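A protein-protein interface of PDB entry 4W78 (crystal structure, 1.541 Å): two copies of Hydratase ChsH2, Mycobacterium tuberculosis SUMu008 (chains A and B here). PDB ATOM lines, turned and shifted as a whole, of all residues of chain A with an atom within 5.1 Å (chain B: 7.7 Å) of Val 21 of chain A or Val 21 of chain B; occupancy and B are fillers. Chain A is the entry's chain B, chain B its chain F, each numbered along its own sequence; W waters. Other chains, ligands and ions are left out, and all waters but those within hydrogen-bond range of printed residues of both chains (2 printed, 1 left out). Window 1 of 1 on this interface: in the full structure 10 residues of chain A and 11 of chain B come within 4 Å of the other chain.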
ATOM      1  N   PRO A  17      -4.145  -1.071   6.128  1.00  0.00           N
ATOM      2  CA  PRO A  17      -5.231  -1.937   6.586  1.00  0.00           C
ATOM      3  C   PRO A  17      -5.074  -2.343   8.046  1.00  0.00           C
ATOM      4  O   PRO A  17      -6.101  -2.377   8.727  1.00  0.00           O
ATOM      5  CB  PRO A  17      -5.143  -3.135   5.642  1.00  0.00           C
ATOM      6  CG  PRO A  17      -4.653  -2.493   4.348  1.00  0.00           C
ATOM      7  CD  PRO A  17      -3.606  -1.521   4.832  1.00  0.00           C
ATOM      8  N   THR A  18      -3.861  -2.612   8.528  1.00  0.00           N
ATOM      9  CA  THR A  18      -3.696  -2.958   9.944  1.00  0.00           C
ATOM     10  C   THR A  18      -4.181  -1.845  10.870  1.00  0.00           C
ATOM     11  O   THR A  18      -4.840  -2.119  11.884  1.00  0.00           O
ATOM     12  CB  THR A  18      -2.251  -3.346  10.266  1.00  0.00           C
ATOM     13  OG1 THR A  18      -1.899  -4.485   9.469  1.00  0.00           O
ATOM     14  CG2 THR A  18      -2.089  -3.670  11.766  1.00  0.00           C
ATOM     15  N   PHE A  19      -3.890  -0.593  10.528  1.00  0.00           N
ATOM     16  CA  PHE A  19      -4.363   0.523  11.329  1.00  0.00           C
ATOM     17  C   PHE A  19      -5.884   0.561  11.373  1.00  0.00           C
ATOM     18  O   PHE A  19      -6.473   0.696  12.455  1.00  0.00           O
ATOM     19  CB  PHE A  19      -3.826   1.848  10.759  1.00  0.00           C
ATOM     20  CG  PHE A  19      -4.307   3.039  11.505  1.00  0.00           C
ATOM     21  CD1 PHE A  19      -3.761   3.363  12.737  1.00  0.00           C
ATOM     22  CD2 PHE A  19      -5.335   3.828  11.000  1.00  0.00           C
ATOM     23  CE1 PHE A  19      -4.217   4.467  13.455  1.00  0.00           C
ATOM     24  CE2 PHE A  19      -5.794   4.936  11.708  1.00  0.00           C
ATOM     25  CZ  PHE A  19      -5.237   5.255  12.937  1.00  0.00           C
ATOM     26  N   ILE A  20      -6.508   0.461  10.204  1.00  0.00           N
ATOM     27  CA  ILE A  20      -7.961   0.560  10.115  1.00  0.00           C
ATOM     28  C   ILE A  20      -8.651  -0.563  10.876  1.00  0.00           C
ATOM     29  O   ILE A  20      -9.584  -0.309  11.643  1.00  0.00           O
ATOM     30  CB  ILE A  20      -8.420   0.584   8.659  1.00  0.00           C
ATOM     31  CG1 ILE A  20      -7.765   1.779   7.958  1.00  0.00           C
ATOM     32  CG2 ILE A  20      -9.957   0.655   8.580  1.00  0.00           C
ATOM     33  CD1 ILE A  20      -8.301   2.027   6.556  1.00  0.00           C
ATOM     34  N   VAL A  21      -8.203  -1.791  10.656  1.00  0.00           N
ATOM     35  CA  VAL A  21      -8.799  -2.950  11.314  1.00  0.00           C
ATOM     36  C   VAL A  21      -8.561  -2.942  12.825  1.00  0.00           C
ATOM     37  O   VAL A  21      -9.511  -3.146  13.621  1.00  0.00           O
ATOM     38  CB  VAL A  21      -8.248  -4.234  10.689  1.00  0.00           C
ATOM     39  CG1 VAL A  21      -8.687  -5.468  11.471  1.00  0.00           C
ATOM     40  CG2 VAL A  21      -8.708  -4.370   9.248  1.00  0.00           C
ATOM     41  N   SER A  22      -7.316  -2.720  13.243  1.00  0.00           N
ATOM     42  CA  SER A  22      -6.990  -2.783  14.665  1.00  0.00           C
ATOM     43  C   SER A  22      -7.689  -1.695  15.464  1.00  0.00           C
ATOM     44  O   SER A  22      -8.127  -1.953  16.602  1.00  0.00           O
ATOM     45  CB  SER A  22      -5.475  -2.742  14.889  1.00  0.00           C
ATOM     46  OG  SER A  22      -4.943  -1.511  14.450  1.00  0.00           O
ATOM     47  N   THR A  23      -7.793  -0.488  14.918  1.00  0.00           N
ATOM     48  CA  THR A  23      -8.490   0.568  15.639  1.00  0.00           C
ATOM     49  C   THR A  23      -9.980   0.277  15.732  1.00  0.00           C
ATOM     50  O   THR A  23     -10.584   0.452  16.785  1.00  0.00           O
ATOM     51  CB  THR A  23      -8.250   1.970  15.034  1.00  0.00           C
ATOM     52  OG1 THR A  23      -8.607   1.983  13.636  1.00  0.00           O
ATOM     53  CG2 THR A  23      -6.782   2.399  15.230  1.00  0.00           C
ATOM     54  N   ALA A  24     -10.584  -0.180  14.644  1.00  0.00           N
ATOM     55  CA  ALA A  24     -12.012  -0.469  14.685  1.00  0.00           C
ATOM     56  C   ALA A  24     -12.304  -1.507  15.754  1.00  0.00           C
ATOM     57  O   ALA A  24     -13.214  -1.321  16.589  1.00  0.00           O
ATOM     58  CB  ALA A  24     -12.506  -0.950  13.313  1.00  0.00           C
ATOM     59  N   LEU A  25     -11.539  -2.595  15.762  1.00  0.00           N
ATOM     60  CA  LEU A  25     -11.818  -3.652  16.731  1.00  0.00           C
ATOM     61  C   LEU A  25     -11.449  -3.253  18.158  1.00  0.00           C
ATOM     62  O   LEU A  25     -12.119  -3.683  19.113  1.00  0.00           O
ATOM     63  CB  LEU A  25     -11.195  -4.990  16.320  1.00  0.00           C
ATOM     64  CG  LEU A  25     -12.125  -5.824  15.435  1.00  0.00           C
ATOM     65  CD1 LEU A  25     -12.388  -5.159  14.086  1.00  0.00           C
ATOM     66  CD2 LEU A  25     -11.566  -7.229  15.222  1.00  0.00           C
ATOM     67  N   ALA A  26     -10.435  -2.401  18.322  1.00  0.00           N
ATOM     68  CA  ALA A  26     -10.121  -1.893  19.660  1.00  0.00           C
ATOM     69  C   ALA A  26     -11.194  -0.948  20.188  1.00  0.00           C
ATOM     70  O   ALA A  26     -11.310  -0.750  21.411  1.00  0.00           O
ATOM     71  CB  ALA A  26      -8.766  -1.212  19.696  1.00  0.00           C
ATOM     72  N   HIS A  34     -15.337  -1.824   8.226  1.00  0.00           N
ATOM     73  CA  HIS A  34     -14.005  -1.460   8.712  1.00  0.00           C
ATOM     74  C   HIS A  34     -12.972  -2.563   8.652  1.00  0.00           C
ATOM     75  O   HIS A  34     -11.808  -2.331   8.986  1.00  0.00           O
ATOM     76  CB  HIS A  34     -14.033  -0.891  10.126  1.00  0.00           C
ATOM     77  CG  HIS A  34     -15.174   0.024  10.347  1.00  0.00           C
ATOM     78  ND1 HIS A  34     -15.325   1.202   9.639  1.00  0.00           N
ATOM     79  CD2 HIS A  34     -16.272  -0.099  11.123  1.00  0.00           C
ATOM     80  CE1 HIS A  34     -16.453   1.777   9.992  1.00  0.00           C
ATOM     81  NE2 HIS A  34     -17.039   1.004  10.878  1.00  0.00           N
ATOM     82  N   HIS A  35     -13.369  -3.758   8.234  1.00  0.00           N
ATOM     83  CA  HIS A  35     -12.377  -4.842   8.177  1.00  0.00           C
ATOM     84  C   HIS A  35     -12.617  -5.854   7.057  1.00  0.00           C
ATOM     85  O   HIS A  35     -11.847  -6.797   6.909  1.00  0.00           O
ATOM     86  CB  HIS A  35     -12.324  -5.592   9.511  1.00  0.00           C
ATOM     87  CG  HIS A  35     -13.593  -6.325   9.823  1.00  0.00           C
ATOM     88  ND1 HIS A  35     -14.543  -5.824  10.687  1.00  0.00           N
ATOM     89  CD2 HIS A  35     -14.087  -7.498   9.361  1.00  0.00           C
ATOM     90  CE1 HIS A  35     -15.569  -6.653  10.737  1.00  0.00           C
ATOM     91  NE2 HIS A  35     -15.323  -7.672   9.935  1.00  0.00           N
ATOM     92  N   ILE A  48     -12.257  -0.703   2.665  1.00  0.00           N
ATOM     93  CA  ILE A  48     -12.470  -0.481   4.094  1.00  0.00           C
ATOM     94  C   ILE A  48     -12.084   0.943   4.492  1.00  0.00           C
ATOM     95  O   ILE A  48     -11.253   1.598   3.833  1.00  0.00           O
ATOM     96  CB  ILE A  48     -11.725  -1.499   4.979  1.00  0.00           C
ATOM     97  CG1 ILE A  48     -10.200  -1.333   4.876  1.00  0.00           C
ATOM     98  CG2 ILE A  48     -12.146  -2.918   4.614  1.00  0.00           C
ATOM     99  CD1 ILE A  48      -9.430  -2.195   5.937  1.00  0.00           C
ATOM    100  N   GLY B  15     -16.032 -19.456   7.266  1.00  0.00           N
ATOM    101  CA  GLY B  15     -14.944 -18.523   7.495  1.00  0.00           C
ATOM    102  C   GLY B  15     -15.103 -17.225   6.732  1.00  0.00           C
ATOM    103  O   GLY B  15     -14.331 -16.939   5.818  1.00  0.00           O
ATOM    104  N   ASP B  16     -16.108 -16.434   7.089  1.00  0.00           N
ATOM    105  CA  ASP B  16     -16.220 -15.130   6.458  1.00  0.00           C
ATOM    106  C   ASP B  16     -15.141 -14.201   7.021  1.00  0.00           C
ATOM    107  O   ASP B  16     -14.511 -14.511   8.039  1.00  0.00           O
ATOM    108  CB  ASP B  16     -17.652 -14.564   6.507  1.00  0.00           C
ATOM    109  CG  ASP B  16     -18.130 -14.198   7.895  1.00  0.00           C
ATOM    110  OD1 ASP B  16     -17.342 -14.170   8.857  1.00  0.00           O
ATOM    111  OD2 ASP B  16     -19.342 -13.895   8.003  1.00  0.00           O
ATOM    112  N   PRO B  17     -14.877 -13.086   6.337  1.00  0.00           N
ATOM    113  CA  PRO B  17     -13.782 -12.236   6.822  1.00  0.00           C
ATOM    114  C   PRO B  17     -13.972 -11.767   8.261  1.00  0.00           C
ATOM    115  O   PRO B  17     -12.983 -11.692   8.994  1.00  0.00           O
ATOM    116  CB  PRO B  17     -13.798 -11.064   5.833  1.00  0.00           C
ATOM    117  CG  PRO B  17     -14.313 -11.671   4.575  1.00  0.00           C
ATOM    118  CD  PRO B  17     -15.354 -12.662   5.007  1.00  0.00           C
ATOM    119  N   THR B  18     -15.205 -11.483   8.679  1.00  0.00           N
ATOM    120  CA  THR B  18     -15.413 -11.089  10.075  1.00  0.00           C
ATOM    121  C   THR B  18     -14.934 -12.161  11.061  1.00  0.00           C
ATOM    122  O   THR B  18     -14.292 -11.843  12.062  1.00  0.00           O
ATOM    123  CB  THR B  18     -16.880 -10.720  10.337  1.00  0.00           C
ATOM    124  OG1 THR B  18     -17.215  -9.589   9.521  1.00  0.00           O
ATOM    125  CG2 THR B  18     -17.091 -10.367  11.787  1.00  0.00           C
ATOM    126  N   PHE B  19     -15.223 -13.421  10.757  1.00  0.00           N
ATOM    127  CA  PHE B  19     -14.755 -14.517  11.591  1.00  0.00           C
ATOM    128  C   PHE B  19     -13.228 -14.559  11.639  1.00  0.00           C
ATOM    129  O   PHE B  19     -12.642 -14.614  12.713  1.00  0.00           O
ATOM    130  CB  PHE B  19     -15.333 -15.835  11.080  1.00  0.00           C
ATOM    131  CG  PHE B  19     -14.867 -17.033  11.831  1.00  0.00           C
ATOM    132  CD1 PHE B  19     -15.426 -17.343  13.059  1.00  0.00           C
ATOM    133  CD2 PHE B  19     -13.860 -17.851  11.321  1.00  0.00           C
ATOM    134  CE1 PHE B  19     -15.000 -18.444  13.777  1.00  0.00           C
ATOM    135  CE2 PHE B  19     -13.436 -18.965  12.030  1.00  0.00           C
ATOM    136  CZ  PHE B  19     -14.002 -19.260  13.256  1.00  0.00           C
ATOM    137  N   ILE B  20     -12.595 -14.505  10.474  1.00  0.00           N
ATOM    138  CA  ILE B  20     -11.145 -14.637  10.400  1.00  0.00           C
ATOM    139  C   ILE B  20     -10.459 -13.477  11.111  1.00  0.00           C
ATOM    140  O   ILE B  20      -9.526 -13.679  11.895  1.00  0.00           O
ATOM    141  CB  ILE B  20     -10.697 -14.719   8.937  1.00  0.00           C
ATOM    142  CG1 ILE B  20     -11.314 -15.959   8.289  1.00  0.00           C
ATOM    143  CG2 ILE B  20      -9.157 -14.721   8.847  1.00  0.00           C
ATOM    144  CD1 ILE B  20     -10.823 -16.246   6.865  1.00  0.00           C
ATOM    145  N   VAL B  21     -10.944 -12.264  10.870  1.00  0.00           N
ATOM    146  CA  VAL B  21     -10.324 -11.073  11.475  1.00  0.00           C
ATOM    147  C   VAL B  21     -10.565 -11.016  12.979  1.00  0.00           C
ATOM    148  O   VAL B  21      -9.630 -10.812  13.768  1.00  0.00           O
ATOM    149  CB  VAL B  21     -10.827  -9.793  10.800  1.00  0.00           C
ATOM    150  CG1 VAL B  21     -10.326  -8.562  11.525  1.00  0.00           C
ATOM    151  CG2 VAL B  21     -10.399  -9.768   9.330  1.00  0.00           C
ATOM    152  N   SER B  22     -11.817 -11.217  13.388  1.00  0.00           N
ATOM    153  CA  SER B  22     -12.148 -11.110  14.806  1.00  0.00           C
ATOM    154  C   SER B  22     -11.453 -12.178  15.645  1.00  0.00           C
ATOM    155  O   SER B  22     -11.010 -11.879  16.750  1.00  0.00           O
ATOM    156  CB  SER B  22     -13.667 -11.112  15.030  1.00  0.00           C
ATOM    157  OG  SER B  22     -14.244 -12.346  14.652  1.00  0.00           O
ATOM    158  N   THR B  23     -11.359 -13.406  15.137  1.00  0.00           N
ATOM    159  CA  THR B  23     -10.640 -14.442  15.873  1.00  0.00           C
ATOM    160  C   THR B  23      -9.145 -14.139  15.948  1.00  0.00           C
ATOM    161  O   THR B  23      -8.542 -14.239  17.016  1.00  0.00           O
ATOM    162  CB  THR B  23     -10.866 -15.845  15.308  1.00  0.00           C
ATOM    163  OG1 THR B  23     -10.543 -15.889  13.917  1.00  0.00           O
ATOM    164  CG2 THR B  23     -12.332 -16.274  15.502  1.00  0.00           C
ATOM    165  N   ALA B  24      -8.557 -13.724  14.834  1.00  0.00           N
ATOM    166  CA  ALA B  24      -7.141 -13.397  14.874  1.00  0.00           C
ATOM    167  C   ALA B  24      -6.854 -12.320  15.905  1.00  0.00           C
ATOM    168  O   ALA B  24      -5.938 -12.485  16.722  1.00  0.00           O
ATOM    169  CB  ALA B  24      -6.638 -12.963  13.493  1.00  0.00           C
ATOM    170  N   LEU B  25      -7.623 -11.234  15.895  1.00  0.00           N
ATOM    171  CA  LEU B  25      -7.336 -10.139  16.825  1.00  0.00           C
ATOM    172  C   LEU B  25      -7.683 -10.486  18.274  1.00  0.00           C
ATOM    173  O   LEU B  25      -7.013 -10.004  19.187  1.00  0.00           O
ATOM    174  CB  LEU B  25      -7.959  -8.805  16.385  1.00  0.00           C
ATOM    175  CG  LEU B  25      -7.036  -8.009  15.457  1.00  0.00           C
ATOM    176  CD1 LEU B  25      -6.743  -8.720  14.141  1.00  0.00           C
ATOM    177  CD2 LEU B  25      -7.608  -6.631  15.229  1.00  0.00           C
ATOM    178  N   ALA B  26      -8.693 -11.331  18.475  1.00  0.00           N
ATOM    179  CA  ALA B  26      -9.016 -11.776  19.831  1.00  0.00           C
ATOM    180  C   ALA B  26      -7.932 -12.703  20.375  1.00  0.00           C
ATOM    181  O   ALA B  26      -7.825 -12.888  21.592  1.00  0.00           O
ATOM    182  CB  ALA B  26     -10.387 -12.475  19.878  1.00  0.00           C
ATOM    183  N   THR B  27      -7.141 -13.317  19.494  1.00  0.00           N
ATOM    184  CA  THR B  27      -5.993 -14.103  19.967  1.00  0.00           C
ATOM    185  C   THR B  27      -4.733 -13.233  20.032  1.00  0.00           C
ATOM    186  O   THR B  27      -3.640 -13.736  20.281  1.00  0.00           O
ATOM    187  CB  THR B  27      -5.708 -15.357  19.109  1.00  0.00           C
ATOM    188  OG1 THR B  27      -5.290 -14.952  17.793  1.00  0.00           O
ATOM    189  CG2 THR B  27      -6.934 -16.239  18.979  1.00  0.00           C
ATOM    190  N   ASP B  29      -3.140 -11.745  17.681  1.00  0.00           N
ATOM    191  CA  ASP B  29      -2.281 -12.000  16.539  1.00  0.00           C
ATOM    192  C   ASP B  29      -2.575 -10.945  15.490  1.00  0.00           C
ATOM    193  O   ASP B  29      -3.631 -10.978  14.841  1.00  0.00           O
ATOM    194  CB  ASP B  29      -2.599 -13.391  15.999  1.00  0.00           C
ATOM    195  CG  ASP B  29      -1.703 -13.807  14.884  1.00  0.00           C
ATOM    196  OD1 ASP B  29      -1.037 -12.949  14.256  1.00  0.00           O
ATOM    197  OD2 ASP B  29      -1.665 -15.026  14.622  1.00  0.00           O
ATOM    198  N   PHE B  30      -1.645  -9.998  15.360  1.00  0.00           N
ATOM    199  CA  PHE B  30      -1.805  -8.872  14.450  1.00  0.00           C
ATOM    200  C   PHE B  30      -1.041  -9.052  13.151  1.00  0.00           C
ATOM    201  O   PHE B  30      -0.852  -8.100  12.394  1.00  0.00           O
ATOM    202  CB  PHE B  30      -1.408  -7.568  15.149  1.00  0.00           C
ATOM    203  CG  PHE B  30      -2.362  -7.171  16.231  1.00  0.00           C
ATOM    204  CD1 PHE B  30      -2.204  -7.649  17.518  1.00  0.00           C
ATOM    205  CD2 PHE B  30      -3.442  -6.334  15.951  1.00  0.00           C
ATOM    206  CE1 PHE B  30      -3.114  -7.305  18.520  1.00  0.00           C
ATOM    207  CE2 PHE B  30      -4.337  -5.980  16.935  1.00  0.00           C
ATOM    208  CZ  PHE B  30      -4.173  -6.468  18.220  1.00  0.00           C
ATOM    209  N   HIS B  34      -3.668 -12.260   8.364  1.00  0.00           N
ATOM    210  CA  HIS B  34      -4.981 -12.690   8.841  1.00  0.00           C
ATOM    211  C   HIS B  34      -6.061 -11.622   8.698  1.00  0.00           C
ATOM    212  O   HIS B  34      -7.238 -11.896   8.957  1.00  0.00           O
ATOM    213  CB  HIS B  34      -4.923 -13.144  10.311  1.00  0.00           C
ATOM    214  CG  HIS B  34      -3.804 -14.089  10.598  1.00  0.00           C
ATOM    215  ND1 HIS B  34      -3.654 -15.298   9.949  1.00  0.00           N
ATOM    216  CD2 HIS B  34      -2.755 -13.982  11.442  1.00  0.00           C
ATOM    217  CE1 HIS B  34      -2.557 -15.893  10.379  1.00  0.00           C
ATOM    218  NE2 HIS B  34      -1.991 -15.110  11.274  1.00  0.00           N
ATOM    219  N   HIS B  35      -5.688 -10.407   8.297  1.00  0.00           N
ATOM    220  CA  HIS B  35      -6.687  -9.347   8.158  1.00  0.00           C
ATOM    221  C   HIS B  35      -6.444  -8.404   6.978  1.00  0.00           C
ATOM    222  O   HIS B  35      -7.292  -7.571   6.668  1.00  0.00           O
ATOM    223  CB  HIS B  35      -6.780  -8.525   9.441  1.00  0.00           C
ATOM    224  CG  HIS B  35      -5.521  -7.780   9.754  1.00  0.00           C
ATOM    225  ND1 HIS B  35      -4.593  -8.253  10.655  1.00  0.00           N
ATOM    226  CD2 HIS B  35      -5.022  -6.617   9.269  1.00  0.00           C
ATOM    227  CE1 HIS B  35      -3.577  -7.408  10.714  1.00  0.00           C
ATOM    228  NE2 HIS B  35      -3.810  -6.411   9.878  1.00  0.00           N
ATOM    229  N   ASP B  36      -5.291  -8.519   6.325  1.00  0.00           N
ATOM    230  CA  ASP B  36      -4.951  -7.653   5.208  1.00  0.00           C
ATOM    231  C   ASP B  36      -4.805  -8.543   3.973  1.00  0.00           C
ATOM    232  O   ASP B  36      -3.794  -9.220   3.803  1.00  0.00           O
ATOM    233  CB  ASP B  36      -3.628  -6.933   5.529  1.00  0.00           C
ATOM    234  CG  ASP B  36      -3.176  -5.967   4.441  1.00  0.00           C
ATOM    235  OD1 ASP B  36      -3.600  -6.096   3.274  1.00  0.00           O
ATOM    236  OD2 ASP B  36      -2.358  -5.068   4.757  1.00  0.00           O
ATOM    237  N   ILE B  48      -6.824 -13.691   2.954  1.00  0.00           N
ATOM    238  CA  ILE B  48      -6.601 -13.823   4.382  1.00  0.00           C
ATOM    239  C   ILE B  48      -6.992 -15.234   4.829  1.00  0.00           C
ATOM    240  O   ILE B  48      -7.829 -15.890   4.209  1.00  0.00           O
ATOM    241  CB  ILE B  48      -7.388 -12.783   5.189  1.00  0.00           C
ATOM    242  CG1 ILE B  48      -8.893 -12.942   4.986  1.00  0.00           C
ATOM    243  CG2 ILE B  48      -6.922 -11.365   4.795  1.00  0.00           C
ATOM    244  CD1 ILE B  48      -9.715 -12.081   5.946  1.00  0.00           C
ATOM    245  N   PHE B  49      -6.348 -15.695   5.895  1.00  0.00           N
ATOM    246  CA  PHE B  49      -6.572 -17.056   6.368  1.00  0.00           C
ATOM    247  C   PHE B  49      -6.517 -17.102   7.883  1.00  0.00           C
ATOM    248  O   PHE B  49      -5.893 -16.257   8.534  1.00  0.00           O
ATOM    249  CB  PHE B  49      -5.579 -18.054   5.748  1.00  0.00           C
ATOM    250  CG  PHE B  49      -4.132 -17.692   5.940  1.00  0.00           C
ATOM    251  CD1 PHE B  49      -3.438 -18.098   7.080  1.00  0.00           C
ATOM    252  CD2 PHE B  49      -3.452 -16.978   4.965  1.00  0.00           C
ATOM    253  CE1 PHE B  49      -2.095 -17.782   7.247  1.00  0.00           C
ATOM    254  CE2 PHE B  49      -2.111 -16.654   5.130  1.00  0.00           C
ATOM    255  CZ  PHE B  49      -1.433 -17.060   6.266  1.00  0.00           C
ATOM    256  N   VAL B  50      -7.189 -18.117   8.415  1.00  0.00           N
ATOM    257  CA  VAL B  50      -7.317 -18.307   9.862  1.00  0.00           C
ATOM    258  C   VAL B  50      -5.964 -18.621  10.495  1.00  0.00           C
ATOM    259  O   VAL B  50      -5.165 -19.381   9.932  1.00  0.00           O
ATOM    260  CB  VAL B  50      -8.312 -19.461  10.124  1.00  0.00           C
ATOM    261  CG1 VAL B  50      -8.378 -19.834  11.618  1.00  0.00           C
ATOM    262  CG2 VAL B  50      -9.699 -19.102   9.622  1.00  0.00           C
ATOM    263  N   ASN B  51      -5.708 -18.054  11.680  1.00  0.00           N
ATOM    264  CA  ASN B  51      -4.414 -18.254  12.353  1.00  0.00           C
ATOM    265  C   ASN B  51      -4.401 -19.506  13.232  1.00  0.00           C
ATOM    266  O   ASN B  51      -5.449 -20.113  13.490  1.00  0.00           O
ATOM    267  CB  ASN B  51      -3.988 -17.007  13.154  1.00  0.00           C
ATOM    268  CG  ASN B  51      -4.759 -16.839  14.468  1.00  0.00           C
ATOM    269  OD1 ASN B  51      -5.860 -17.346  14.620  1.00  0.00           O
ATOM    270  ND2 ASN B  51      -4.159 -16.143  15.425  1.00  0.00           N
ATOM    271  N   THR B  54      -6.358 -19.588  16.595  1.00  0.00           N
ATOM    272  CA  THR B  54      -7.786 -19.810  16.398  1.00  0.00           C
ATOM    273  C   THR B  54      -8.065 -21.287  16.104  1.00  0.00           C
ATOM    274  O   THR B  54      -9.033 -21.841  16.621  1.00  0.00           O
ATOM    275  CB  THR B  54      -8.329 -18.913  15.271  1.00  0.00           C
ATOM    276  OG1 THR B  54      -8.232 -17.544  15.691  1.00  0.00           O
ATOM    277  CG2 THR B  54      -9.771 -19.258  14.934  1.00  0.00           C
HETATM  278  O   HOH W   1     -10.093  -8.317   5.921  1.00  0.00           O
HETATM  279  O   HOH W   2      -9.001  -5.840   5.958  1.00  0.00           O
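NE2 of His 35 of chain B sits at hydrogen-bond distance from OG1 of Thr 18 of chain A, 2.7 Å away.
NE2 of His 35 of chain A lies within hydrogen-bond range of OG1 of Thr 18 of chain B (2.7 Å).
The backbone carbonyl oxygen (O) of Thr 18 of chain A sits at hydrogen-bond distance from the side-chain hydroxyl (OG) of Ser 22 of chain A (2.6 Å).
The backbone carbonyl oxygen (O) of Phe 19 of chain A lies within hydrogen-bond range of the side-chain hydroxyl (OG) of Ser 22 of chain A (3.3 Å).
OD1 of Asp 16 of chain B lies close to N of Thr 18 of chain B (3.4 Å).
The side-chain hydroxyl of Ser 22 of chain B lies within hydrogen-bond range of the backbone carbonyl oxygen of Thr 18 of chain B (2.6 Å).
O of Phe 19 of chain B sits at hydrogen-bond distance from OG of Ser 22 of chain B (3.4 Å).
OD2 of Asp 36 of chain B touches CG of Pro 17 of chain A, at 3.5 Å.
Val 21 of chain A touches Val 21 of chain B.
Ser 22 of chain A touches Leu 25 of chain B.
CB of Ser 22 of chain A touches CE2 of Phe 30 of chain B, at 3.996 Å.
CD2 of Leu 25 of chain A touches CA of Ser 22 of chain B, at 3.9 Å.
Of chain B, only Val 21 (3.5 Å) comes within 4 Å of Val 21 of chain A.
Printed residues of chain B within 4 Å of Ser 22 of chain A: Leu 25 (3.9 Å) and Phe 30 (3.996 Å).
Printed residues of chain A within 4 Å of Thr 18 of chain B: His 35.
Of chain A, only Val 21 (3.5 Å) comes within 4 Å of Val 21 of chain B.
Printed residues of chain A within 4 Å of Leu 25 of chain B: Ser 22 (3.9 Å).
Of the printed residues of chain A, Phe 30 of chain B touches Ser 22 (3.996 Å).
Of the printed residues of chain A, Asp 36 of chain B touches Pro 17 (3.5 Å).
Of the 13 printed residues of chain A, 6 touch a printed residue of chain B.
Hydrophobic or aromatic side chains of chain A that line the printed part of chain B: Pro 17, Val 21, Leu 25 and His 35.
Thr 18 of chain A touches His 35 of chain B, and with the chains exchanged His 35 of chain A touches Thr 18 of chain B.
Val 21 of chain B touches its own counterpart, Val 21 of chain A.
Ser 22 of chain A touches Leu 25 of chain B, and with the chains exchanged Leu 25 of chain A touches Ser 22 of chain B.
Water W1 bridges the backbone carbonyl oxygen of His 35 of chain A and the backbone carbonyl oxygen of His 35 of chain B.
Water W2 lies within hydrogen-bond range of O of His 35 of chain B (2.5 Å) and O of His 35 of chain A (3.1 Å).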
